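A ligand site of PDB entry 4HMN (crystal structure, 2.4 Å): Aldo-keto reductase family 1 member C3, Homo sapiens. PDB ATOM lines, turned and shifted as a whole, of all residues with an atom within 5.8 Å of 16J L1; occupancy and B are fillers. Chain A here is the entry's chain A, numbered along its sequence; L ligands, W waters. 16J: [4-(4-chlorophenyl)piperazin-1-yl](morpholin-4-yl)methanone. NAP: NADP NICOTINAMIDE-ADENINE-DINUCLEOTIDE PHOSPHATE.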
ATOM      1  N   TYR A  24      24.014  -1.005  14.690  1.00  0.00           N
ATOM      2  CA  TYR A  24      22.825  -0.731  13.878  1.00  0.00           C
ATOM      3  C   TYR A  24      22.806  -1.470  12.514  1.00  0.00           C
ATOM      4  O   TYR A  24      23.812  -1.470  11.729  1.00  0.00           O
ATOM      5  CB  TYR A  24      22.597   0.795  13.636  1.00  0.00           C
ATOM      6  CG  TYR A  24      21.251   1.030  12.966  1.00  0.00           C
ATOM      7  CD1 TYR A  24      20.065   0.944  13.726  1.00  0.00           C
ATOM      8  CD2 TYR A  24      21.129   1.213  11.577  1.00  0.00           C
ATOM      9  CE1 TYR A  24      18.813   1.099  13.143  1.00  0.00           C
ATOM     10  CE2 TYR A  24      19.837   1.360  10.987  1.00  0.00           C
ATOM     11  CZ  TYR A  24      18.703   1.302  11.803  1.00  0.00           C
ATOM     12  OH  TYR A  24      17.422   1.454  11.327  1.00  0.00           O
ATOM     13  N   ALA A  52      21.356   0.990  21.235  1.00  0.00           N
ATOM     14  CA  ALA A  52      20.408   2.045  21.591  1.00  0.00           C
ATOM     15  C   ALA A  52      19.011   1.462  21.551  1.00  0.00           C
ATOM     16  O   ALA A  52      18.801   0.376  21.000  1.00  0.00           O
ATOM     17  CB  ALA A  52      20.505   3.237  20.632  1.00  0.00           C
ATOM     18  N   LEU A  54      16.360   2.916  20.142  1.00  0.00           N
ATOM     19  CA  LEU A  54      16.016   3.080  18.714  1.00  0.00           C
ATOM     20  C   LEU A  54      16.376   1.879  17.839  1.00  0.00           C
ATOM     21  O   LEU A  54      15.629   1.549  16.955  1.00  0.00           O
ATOM     22  CB  LEU A  54      16.649   4.351  18.116  1.00  0.00           C
ATOM     23  CG  LEU A  54      16.017   4.776  16.773  1.00  0.00           C
ATOM     24  CD1 LEU A  54      14.700   5.493  16.950  1.00  0.00           C
ATOM     25  CD2 LEU A  54      16.976   5.622  15.949  1.00  0.00           C
ATOM     26  N   TYR A  55      17.500   1.233  18.091  1.00  0.00           N
ATOM     27  CA  TYR A  55      18.043   0.216  17.155  1.00  0.00           C
ATOM     28  C   TYR A  55      17.277  -1.092  17.185  1.00  0.00           C
ATOM     29  O   TYR A  55      17.480  -1.896  16.301  1.00  0.00           O
ATOM     30  CB  TYR A  55      19.535  -0.093  17.423  1.00  0.00           C
ATOM     31  CG  TYR A  55      20.470   1.102  17.406  1.00  0.00           C
ATOM     32  CD1 TYR A  55      20.074   2.326  16.873  1.00  0.00           C
ATOM     33  CD2 TYR A  55      21.770   1.012  17.949  1.00  0.00           C
ATOM     34  CE1 TYR A  55      20.904   3.401  16.893  1.00  0.00           C
ATOM     35  CE2 TYR A  55      22.613   2.105  17.975  1.00  0.00           C
ATOM     36  CZ  TYR A  55      22.164   3.304  17.428  1.00  0.00           C
ATOM     37  OH  TYR A  55      22.972   4.438  17.400  1.00  0.00           O
ATOM     38  N   LYS A  84      21.341   3.962  24.842  1.00  0.00           N
ATOM     39  CA  LYS A  84      21.026   5.369  24.713  1.00  0.00           C
ATOM     40  C   LYS A  84      19.558   5.634  24.968  1.00  0.00           C
ATOM     41  O   LYS A  84      18.675   4.818  24.598  1.00  0.00           O
ATOM     42  CB  LYS A  84      21.416   5.867  23.331  1.00  0.00           C
ATOM     43  CG  LYS A  84      22.753   5.339  22.791  1.00  0.00           C
ATOM     44  CD  LYS A  84      23.264   6.161  21.611  1.00  0.00           C
ATOM     45  CE  LYS A  84      24.458   5.499  20.879  1.00  0.00           C
ATOM     46  NZ  LYS A  84      24.087   4.300  20.050  1.00  0.00           N
ATOM     47  N   TRP A  86      16.451   7.264  24.109  1.00  0.00           N
ATOM     48  CA  TRP A  86      15.722   7.851  23.012  1.00  0.00           C
ATOM     49  C   TRP A  86      14.974   9.131  23.353  1.00  0.00           C
ATOM     50  O   TRP A  86      14.628   9.346  24.504  1.00  0.00           O
ATOM     51  CB  TRP A  86      14.804   6.831  22.339  1.00  0.00           C
ATOM     52  CG  TRP A  86      14.232   7.410  21.062  1.00  0.00           C
ATOM     53  CD1 TRP A  86      12.884   7.545  20.734  1.00  0.00           C
ATOM     54  CD2 TRP A  86      14.960   8.073  19.950  1.00  0.00           C
ATOM     55  NE1 TRP A  86      12.734   8.177  19.505  1.00  0.00           N
ATOM     56  CE2 TRP A  86      13.950   8.526  18.986  1.00  0.00           C
ATOM     57  CE3 TRP A  86      16.303   8.309  19.657  1.00  0.00           C
ATOM     58  CZ2 TRP A  86      14.289   9.165  17.803  1.00  0.00           C
ATOM     59  CZ3 TRP A  86      16.626   8.962  18.451  1.00  0.00           C
ATOM     60  CH2 TRP A  86      15.634   9.393  17.560  1.00  0.00           C
ATOM     61  N   HIS A 117      20.578  10.266  23.573  1.00  0.00           N
ATOM     62  CA  HIS A 117      20.797   9.928  22.152  1.00  0.00           C
ATOM     63  C   HIS A 117      20.920  11.182  21.280  1.00  0.00           C
ATOM     64  O   HIS A 117      21.677  11.171  20.291  1.00  0.00           O
ATOM     65  CB  HIS A 117      19.630   9.034  21.661  1.00  0.00           C
ATOM     66  CG  HIS A 117      19.976   8.124  20.491  1.00  0.00           C
ATOM     67  ND1 HIS A 117      19.470   6.871  20.388  1.00  0.00           N
ATOM     68  CD2 HIS A 117      20.801   8.325  19.372  1.00  0.00           C
ATOM     69  CE1 HIS A 117      19.971   6.292  19.257  1.00  0.00           C
ATOM     70  NE2 HIS A 117      20.775   7.179  18.646  1.00  0.00           N
ATOM     71  N   SER A 118      20.214  12.246  21.655  1.00  0.00           N
ATOM     72  CA  SER A 118      20.012  13.438  20.795  1.00  0.00           C
ATOM     73  C   SER A 118      19.391  14.540  21.645  1.00  0.00           C
ATOM     74  O   SER A 118      18.594  14.240  22.567  1.00  0.00           O
ATOM     75  CB  SER A 118      19.047  13.092  19.652  1.00  0.00           C
ATOM     76  OG  SER A 118      18.701  14.179  18.827  1.00  0.00           O
ATOM     77  N   PRO A 119      19.737  15.811  21.352  1.00  0.00           N
ATOM     78  CA  PRO A 119      19.123  16.953  22.056  1.00  0.00           C
ATOM     79  C   PRO A 119      17.722  17.324  21.508  1.00  0.00           C
ATOM     80  O   PRO A 119      17.030  18.164  22.073  1.00  0.00           O
ATOM     81  CB  PRO A 119      20.130  18.104  21.818  1.00  0.00           C
ATOM     82  CG  PRO A 119      20.835  17.739  20.545  1.00  0.00           C
ATOM     83  CD  PRO A 119      20.854  16.233  20.476  1.00  0.00           C
ATOM     84  N   MET A 120      17.307  16.698  20.423  1.00  0.00           N
ATOM     85  CA  MET A 120      16.099  17.106  19.742  1.00  0.00           C
ATOM     86  C   MET A 120      14.926  16.343  20.355  1.00  0.00           C
ATOM     87  O   MET A 120      14.622  15.228  19.960  1.00  0.00           O
ATOM     88  CB  MET A 120      16.241  16.895  18.230  1.00  0.00           C
ATOM     89  CG  MET A 120      17.224  17.873  17.566  1.00  0.00           C
ATOM     90  SD  MET A 120      17.431  17.512  15.799  1.00  0.00           S
ATOM     91  CE  MET A 120      18.547  16.110  16.024  1.00  0.00           C
ATOM     92  N   ASN A 167      25.175  13.738  19.998  1.00  0.00           N
ATOM     93  CA  ASN A 167      24.634  14.705  19.057  1.00  0.00           C
ATOM     94  C   ASN A 167      24.476  16.105  19.586  1.00  0.00           C
ATOM     95  O   ASN A 167      23.694  16.903  19.045  1.00  0.00           O
ATOM     96  CB  ASN A 167      23.344  14.171  18.490  1.00  0.00           C
ATOM     97  CG  ASN A 167      23.603  13.032  17.543  1.00  0.00           C
ATOM     98  OD1 ASN A 167      24.347  13.221  16.587  1.00  0.00           O
ATOM     99  ND2 ASN A 167      23.058  11.855  17.830  1.00  0.00           N
ATOM    100  N   TYR A 216      30.709   8.379  15.364  1.00  0.00           N
ATOM    101  CA  TYR A 216      29.856   7.495  14.546  1.00  0.00           C
ATOM    102  C   TYR A 216      29.844   7.886  13.057  1.00  0.00           C
ATOM    103  O   TYR A 216      30.261   8.985  12.675  1.00  0.00           O
ATOM    104  CB  TYR A 216      28.428   7.417  15.101  1.00  0.00           C
ATOM    105  CG  TYR A 216      27.514   8.609  14.892  1.00  0.00           C
ATOM    106  CD1 TYR A 216      27.049   8.949  13.652  1.00  0.00           C
ATOM    107  CD2 TYR A 216      27.045   9.354  15.981  1.00  0.00           C
ATOM    108  CE1 TYR A 216      26.183  10.008  13.477  1.00  0.00           C
ATOM    109  CE2 TYR A 216      26.202  10.438  15.819  1.00  0.00           C
ATOM    110  CZ  TYR A 216      25.764  10.747  14.575  1.00  0.00           C
ATOM    111  OH  TYR A 216      24.935  11.803  14.394  1.00  0.00           O
ATOM    112  N   GLN A 222      25.931   4.286   6.714  1.00  0.00           N
ATOM    113  CA  GLN A 222      25.384   3.205   5.892  1.00  0.00           C
ATOM    114  C   GLN A 222      24.539   3.710   4.714  1.00  0.00           C
ATOM    115  O   GLN A 222      23.961   2.893   3.982  1.00  0.00           O
ATOM    116  CB  GLN A 222      24.560   2.239   6.772  1.00  0.00           C
ATOM    117  CG  GLN A 222      25.334   1.708   7.964  1.00  0.00           C
ATOM    118  CD  GLN A 222      24.548   0.670   8.780  1.00  0.00           C
ATOM    119  OE1 GLN A 222      24.032  -0.305   8.227  1.00  0.00           O
ATOM    120  NE2 GLN A 222      24.487   0.869  10.096  1.00  0.00           N
ATOM    121  N   ASP A 224      21.572   5.266   4.389  1.00  0.00           N
ATOM    122  CA  ASP A 224      20.161   4.888   4.452  1.00  0.00           C
ATOM    123  C   ASP A 224      19.368   6.032   3.775  1.00  0.00           C
ATOM    124  O   ASP A 224      19.517   7.209   4.117  1.00  0.00           O
ATOM    125  CB  ASP A 224      19.767   4.645   5.940  1.00  0.00           C
ATOM    126  CG  ASP A 224      18.510   3.792   6.104  1.00  0.00           C
ATOM    127  OD1 ASP A 224      17.459   4.305   5.716  1.00  0.00           O
ATOM    128  OD2 ASP A 224      18.574   2.647   6.637  1.00  0.00           O
ATOM    129  N   ARG A 226      16.606   6.997   4.088  1.00  0.00           N
ATOM    130  CA  ARG A 226      15.718   7.742   4.989  1.00  0.00           C
ATOM    131  C   ARG A 226      16.308   9.036   5.460  1.00  0.00           C
ATOM    132  O   ARG A 226      15.570   9.937   5.770  1.00  0.00           O
ATOM    133  CB  ARG A 226      15.343   6.927   6.215  1.00  0.00           C
ATOM    134  CG  ARG A 226      14.159   5.985   5.983  1.00  0.00           C
ATOM    135  CD  ARG A 226      13.923   5.187   7.253  1.00  0.00           C
ATOM    136  NE  ARG A 226      14.975   4.192   7.470  1.00  0.00           N
ATOM    137  CZ  ARG A 226      15.177   3.545   8.609  1.00  0.00           C
ATOM    138  NH1 ARG A 226      14.389   3.796   9.669  1.00  0.00           N
ATOM    139  NH2 ARG A 226      16.160   2.650   8.695  1.00  0.00           N
ATOM    140  N   TRP A 227      17.628   9.116   5.527  1.00  0.00           N
ATOM    141  CA  TRP A 227      18.335  10.288   6.082  1.00  0.00           C
ATOM    142  C   TRP A 227      19.463  10.826   5.240  1.00  0.00           C
ATOM    143  O   TRP A 227      19.891  11.970   5.492  1.00  0.00           O
ATOM    144  CB  TRP A 227      18.913   9.973   7.486  1.00  0.00           C
ATOM    145  CG  TRP A 227      17.935   9.436   8.496  1.00  0.00           C
ATOM    146  CD1 TRP A 227      16.897  10.118   9.123  1.00  0.00           C
ATOM    147  CD2 TRP A 227      17.860   8.053   9.024  1.00  0.00           C
ATOM    148  NE1 TRP A 227      16.194   9.276   9.966  1.00  0.00           N
ATOM    149  CE2 TRP A 227      16.723   8.026   9.958  1.00  0.00           C
ATOM    150  CE3 TRP A 227      18.581   6.910   8.820  1.00  0.00           C
ATOM    151  CZ2 TRP A 227      16.353   6.891  10.643  1.00  0.00           C
ATOM    152  CZ3 TRP A 227      18.193   5.750   9.514  1.00  0.00           C
ATOM    153  CH2 TRP A 227      17.111   5.743  10.405  1.00  0.00           C
ATOM    154  N   PHE A 306      23.822  12.609   7.703  1.00  0.00           N
ATOM    155  CA  PHE A 306      22.450  12.721   8.215  1.00  0.00           C
ATOM    156  C   PHE A 306      21.983  14.180   8.043  1.00  0.00           C
ATOM    157  O   PHE A 306      22.473  15.099   8.714  1.00  0.00           O
ATOM    158  CB  PHE A 306      22.355  12.283   9.691  1.00  0.00           C
ATOM    159  CG  PHE A 306      22.607  10.800   9.910  1.00  0.00           C
ATOM    160  CD1 PHE A 306      23.881  10.326  10.058  1.00  0.00           C
ATOM    161  CD2 PHE A 306      21.554   9.904   9.926  1.00  0.00           C
ATOM    162  CE1 PHE A 306      24.104   8.969  10.251  1.00  0.00           C
ATOM    163  CE2 PHE A 306      21.754   8.545  10.125  1.00  0.00           C
ATOM    164  CZ  PHE A 306      23.038   8.079  10.281  1.00  0.00           C
ATOM    165  N   PHE A 311      14.972  16.485  11.207  1.00  0.00           N
ATOM    166  CA  PHE A 311      15.848  17.067  12.243  1.00  0.00           C
ATOM    167  C   PHE A 311      16.065  18.544  12.071  1.00  0.00           C
ATOM    168  O   PHE A 311      16.325  19.230  13.062  1.00  0.00           O
ATOM    169  CB  PHE A 311      17.328  16.607  12.147  1.00  0.00           C
ATOM    170  CG  PHE A 311      17.509  15.163  11.991  1.00  0.00           C
ATOM    171  CD1 PHE A 311      16.823  14.260  12.819  1.00  0.00           C
ATOM    172  CD2 PHE A 311      18.403  14.679  11.039  1.00  0.00           C
ATOM    173  CE1 PHE A 311      17.008  12.890  12.664  1.00  0.00           C
ATOM    174  CE2 PHE A 311      18.585  13.320  10.876  1.00  0.00           C
ATOM    175  CZ  PHE A 311      17.879  12.422  11.681  1.00  0.00           C
ATOM    176  N   TYR A 317      18.172  21.548  16.840  1.00  0.00           N
ATOM    177  CA  TYR A 317      19.115  21.060  15.790  1.00  0.00           C
ATOM    178  C   TYR A 317      20.559  21.426  16.141  1.00  0.00           C
ATOM    179  O   TYR A 317      20.887  22.607  16.260  1.00  0.00           O
ATOM    180  CB  TYR A 317      18.711  21.679  14.442  1.00  0.00           C
ATOM    181  CG  TYR A 317      19.387  21.136  13.220  1.00  0.00           C
ATOM    182  CD1 TYR A 317      19.497  19.778  13.012  1.00  0.00           C
ATOM    183  CD2 TYR A 317      19.863  21.976  12.250  1.00  0.00           C
ATOM    184  CE1 TYR A 317      20.089  19.262  11.871  1.00  0.00           C
ATOM    185  CE2 TYR A 317      20.465  21.487  11.093  1.00  0.00           C
ATOM    186  CZ  TYR A 317      20.578  20.119  10.908  1.00  0.00           C
ATOM    187  OH  TYR A 317      21.179  19.588   9.768  1.00  0.00           O
ATOM    188  N   PRO A 318      21.421  20.424  16.346  1.00  0.00           N
ATOM    189  CA  PRO A 318      22.797  20.732  16.743  1.00  0.00           C
ATOM    190  C   PRO A 318      23.684  21.404  15.670  1.00  0.00           C
ATOM    191  O   PRO A 318      24.694  22.066  16.013  1.00  0.00           O
ATOM    192  CB  PRO A 318      23.377  19.342  17.089  1.00  0.00           C
ATOM    193  CG  PRO A 318      22.566  18.392  16.299  1.00  0.00           C
ATOM    194  CD  PRO A 318      21.175  18.966  16.345  1.00  0.00           C
ATOM    195  N   TYR A 319      23.351  21.224  14.393  1.00  0.00           N
ATOM    196  CA  TYR A 319      24.207  21.769  13.316  1.00  0.00           C
ATOM    197  C   TYR A 319      23.741  23.139  12.974  1.00  0.00           C
ATOM    198  O   TYR A 319      24.099  23.665  11.936  1.00  0.00           O
ATOM    199  CB  TYR A 319      24.212  20.880  12.057  1.00  0.00           C
ATOM    200  CG  TYR A 319      24.583  19.443  12.331  1.00  0.00           C
ATOM    201  CD1 TYR A 319      25.663  19.153  13.113  1.00  0.00           C
ATOM    202  CD2 TYR A 319      23.859  18.397  11.808  1.00  0.00           C
ATOM    203  CE1 TYR A 319      26.015  17.851  13.382  1.00  0.00           C
ATOM    204  CE2 TYR A 319      24.211  17.073  12.072  1.00  0.00           C
ATOM    205  CZ  TYR A 319      25.317  16.818  12.879  1.00  0.00           C
ATOM    206  OH  TYR A 319      25.724  15.533  13.226  1.00  0.00           O
HETATM  207  CAI 16J L   1      21.738   4.331  13.795  1.00  0.00           C
HETATM  208  CAG 16J L   1      22.705   4.409  12.590  1.00  0.00           C
HETATM  209  OAO 16J L   1      21.945   4.015  11.363  1.00  0.00           O
HETATM  210  CAH 16J L   1      20.565   4.548  11.349  1.00  0.00           C
HETATM  211  CAJ 16J L   1      20.039   5.548  12.429  1.00  0.00           C
HETATM  212  NAS 16J L   1      20.747   5.434  13.726  1.00  0.00           N
HETATM  213  CAP 16J L   1      20.624   6.315  14.748  1.00  0.00           C
HETATM  214  OAA 16J L   1      21.281   6.147  15.807  1.00  0.00           O
HETATM  215  NAT 16J L   1      19.776   7.351  14.781  1.00  0.00           N
HETATM  216  CAL 16J L   1      18.996   7.901  13.665  1.00  0.00           C
HETATM  217  CAN 16J L   1      19.701   9.258  13.281  1.00  0.00           C
HETATM  218  CAK 16J L   1      19.813   8.197  15.966  1.00  0.00           C
HETATM  219  CAM 16J L   1      19.274   9.613  15.725  1.00  0.00           C
HETATM  220  NAU 16J L   1      19.775  10.166  14.476  1.00  0.00           N
HETATM  221  CAR 16J L   1      20.299  11.481  14.496  1.00  0.00           C
HETATM  222  CAE 16J L   1      19.934  12.396  15.495  1.00  0.00           C
HETATM  223  CAC 16J L   1      20.435  13.688  15.531  1.00  0.00           C
HETATM  224  CAQ 16J L   1      21.344  14.083  14.560  1.00  0.00           C
HETATM  225 CLA  16J L   1      22.022  15.669  14.525  1.00  0.00          CL
HETATM  226  CAD 16J L   1      21.736  13.182  13.582  1.00  0.00           C
HETATM  227  CAF 16J L   1      21.205  11.889  13.545  1.00  0.00           C
HETATM  228  PA  NAP L   2      29.848   3.062   9.744  1.00  0.00           P
HETATM  229  O1A NAP L   2      30.709   2.587  10.821  1.00  0.00           O
HETATM  230  O2A NAP L   2      30.058   4.412   9.278  1.00  0.00           O
HETATM  231  O5B NAP L   2      29.913   1.910   8.531  1.00  0.00           O
HETATM  232  C5B NAP L   2      29.332   2.172   7.253  1.00  0.00           C
HETATM  233  C4B NAP L   2      29.447   0.906   6.321  1.00  0.00           C
HETATM  234  O4B NAP L   2      30.814   0.640   6.276  1.00  0.00           O
HETATM  235  C3B NAP L   2      28.851  -0.238   7.079  1.00  0.00           C
HETATM  236  O3B NAP L   2      27.493  -0.392   6.691  1.00  0.00           O
HETATM  237  C2B NAP L   2      29.720  -1.395   6.688  1.00  0.00           C
HETATM  238  O2B NAP L   2      29.124  -2.208   5.650  1.00  0.00           O
HETATM  239  C1B NAP L   2      30.926  -0.726   6.105  1.00  0.00           C
HETATM  240  N9A NAP L   2      32.264  -1.261   6.602  1.00  0.00           N
HETATM  241  C8A NAP L   2      32.677  -1.672   7.775  1.00  0.00           C
HETATM  242  N7A NAP L   2      33.953  -2.045   7.717  1.00  0.00           N
HETATM  243  C5A NAP L   2      34.354  -1.850   6.468  1.00  0.00           C
HETATM  244  C6A NAP L   2      35.563  -2.086   5.799  1.00  0.00           C
HETATM  245  N6A NAP L   2      36.671  -2.546   6.447  1.00  0.00           N
HETATM  246  N1A NAP L   2      35.634  -1.864   4.440  1.00  0.00           N
HETATM  247  C2A NAP L   2      34.510  -1.391   3.606  1.00  0.00           C
HETATM  248  N3A NAP L   2      33.306  -1.042   4.393  1.00  0.00           N
HETATM  249  C4A NAP L   2      33.261  -1.356   5.775  1.00  0.00           C
HETATM  250  O3  NAP L   2      28.303   2.802  10.007  1.00  0.00           O
HETATM  251  PN  NAP L   2      27.249   3.606  11.027  1.00  0.00           P
HETATM  252  O1N NAP L   2      26.282   2.485  11.306  1.00  0.00           O
HETATM  253  O2N NAP L   2      26.775   4.896  10.444  1.00  0.00           O
HETATM  254  O5D NAP L   2      28.087   3.934  12.318  1.00  0.00           O
HETATM  255  C5D NAP L   2      28.539   2.988  13.248  1.00  0.00           C
HETATM  256  C4D NAP L   2      27.768   2.980  14.636  1.00  0.00           C
HETATM  257  O4D NAP L   2      27.717   4.233  15.414  1.00  0.00           O
HETATM  258  C3D NAP L   2      26.354   2.658  14.296  1.00  0.00           C
HETATM  259  O3D NAP L   2      26.360   1.264  13.954  1.00  0.00           O
HETATM  260  C2D NAP L   2      25.709   2.933  15.656  1.00  0.00           C
HETATM  261  O2D NAP L   2      26.156   1.960  16.623  1.00  0.00           O
HETATM  262  C1D NAP L   2      26.409   4.263  15.998  1.00  0.00           C
HETATM  263  N1N NAP L   2      25.720   5.419  15.421  1.00  0.00           N
HETATM  264  C2N NAP L   2      25.144   6.295  16.312  1.00  0.00           C
HETATM  265  C3N NAP L   2      24.457   7.421  15.915  1.00  0.00           C
HETATM  266  C7N NAP L   2      23.865   8.398  16.939  1.00  0.00           C
HETATM  267  O7N NAP L   2      23.038   9.250  16.612  1.00  0.00           O
HETATM  268  N7N NAP L   2      24.405   8.371  18.161  1.00  0.00           N
HETATM  269  C4N NAP L   2      24.335   7.628  14.560  1.00  0.00           C
HETATM  270  C5N NAP L   2      24.925   6.744  13.642  1.00  0.00           C
HETATM  271  C6N NAP L   2      25.615   5.629  14.052  1.00  0.00           C
HETATM  272  P2B NAP L   2      28.969  -3.802   5.968  1.00  0.00           P
HETATM  273  O1X NAP L   2      28.518  -4.446   4.614  1.00  0.00           O
HETATM  274  O2X NAP L   2      30.472  -4.412   6.262  1.00  0.00           O
HETATM  275  O3X NAP L   2      28.071  -4.064   7.190  1.00  0.00           O
HETATM  276  O   HOH W   1      22.026   3.637   8.785  1.00  0.00           O
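Tyr 24 touches 16J L1 (CD2 to OAO, 2.9 Å). Leu 54 touches 16J L1. Trp 86 touches 16J L1. OG of Ser 118 touches CAC of 16J L1, 3.8 Å away. Met 120 touches 16J L1. Asn 167 touches 16J L1. Tyr 216 touches 16J L1 (OH to CAD, 3.6 Å). Trp 227 touches 16J L1 (CZ3 to CAH, 3.2 Å). Phe 306 touches 16J L1 (CE2 to CAN, 3.8 Å). Phe 311 touches 16J L1. Pro 318 touches 16J L1 (CG to CLA, 3.3 Å). Tyr 319 touches 16J L1. Hydrophobic or aromatic side chains that line 16J L1: Tyr 24, Leu 54, Tyr 55, Trp 86, His 117, Met 120, Trp 227, Phe 306, Phe 311, Pro 318 and Tyr 319. 14 residues have an atom within 4 Å of 16J L1: Tyr 24, Leu 54, Tyr 55, Trp 86, His 117, Ser 118, Met 120, Asn 167, Tyr 216, Trp 227, Phe 306, Phe 311, Pro 318 and Tyr 319.
The side-chain hydroxyl of Tyr 55 lies within hydrogen-bond range of an oxygen (OAA) of 16J L1. An oxygen (OAA) of 16J L1 lies close to a ring nitrogen (NE2) of His 117. O3D of NAP L2 lies within hydrogen-bond range of N of Tyr 24, at 3.3 Å. The side-chain amide nitrogen of Asn 167 lies within hydrogen-bond range of an oxygen (O7N) of NAP L2 (2.9 Å). The side-chain amide nitrogen (NE2) of Gln 222 lies within hydrogen-bond range of an oxygen (O1N) of NAP L2 (2.7 Å).
The side-chain amino group (NZ) of Lys 84 sits at hydrogen-bond distance from the side-chain hydroxyl (OH) of Tyr 55, at 2.9 Å. The backbone carbonyl oxygen of Tyr 24 sits at hydrogen-bond distance from the side-chain amide nitrogen of Gln 222, 2.9 Å away. OH of Tyr 24 is in hydrogen-bond range of NH2 of Arg 226 (3.2 Å). ND2 of Asn 167 lies within hydrogen-bond range of O of His 117 (2.9 Å). N of Met 120 lies close to OG of Ser 118 (3.3 Å). OD1 of Asn 167 is in hydrogen-bond range of OH of Tyr 216 (2.7 Å).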
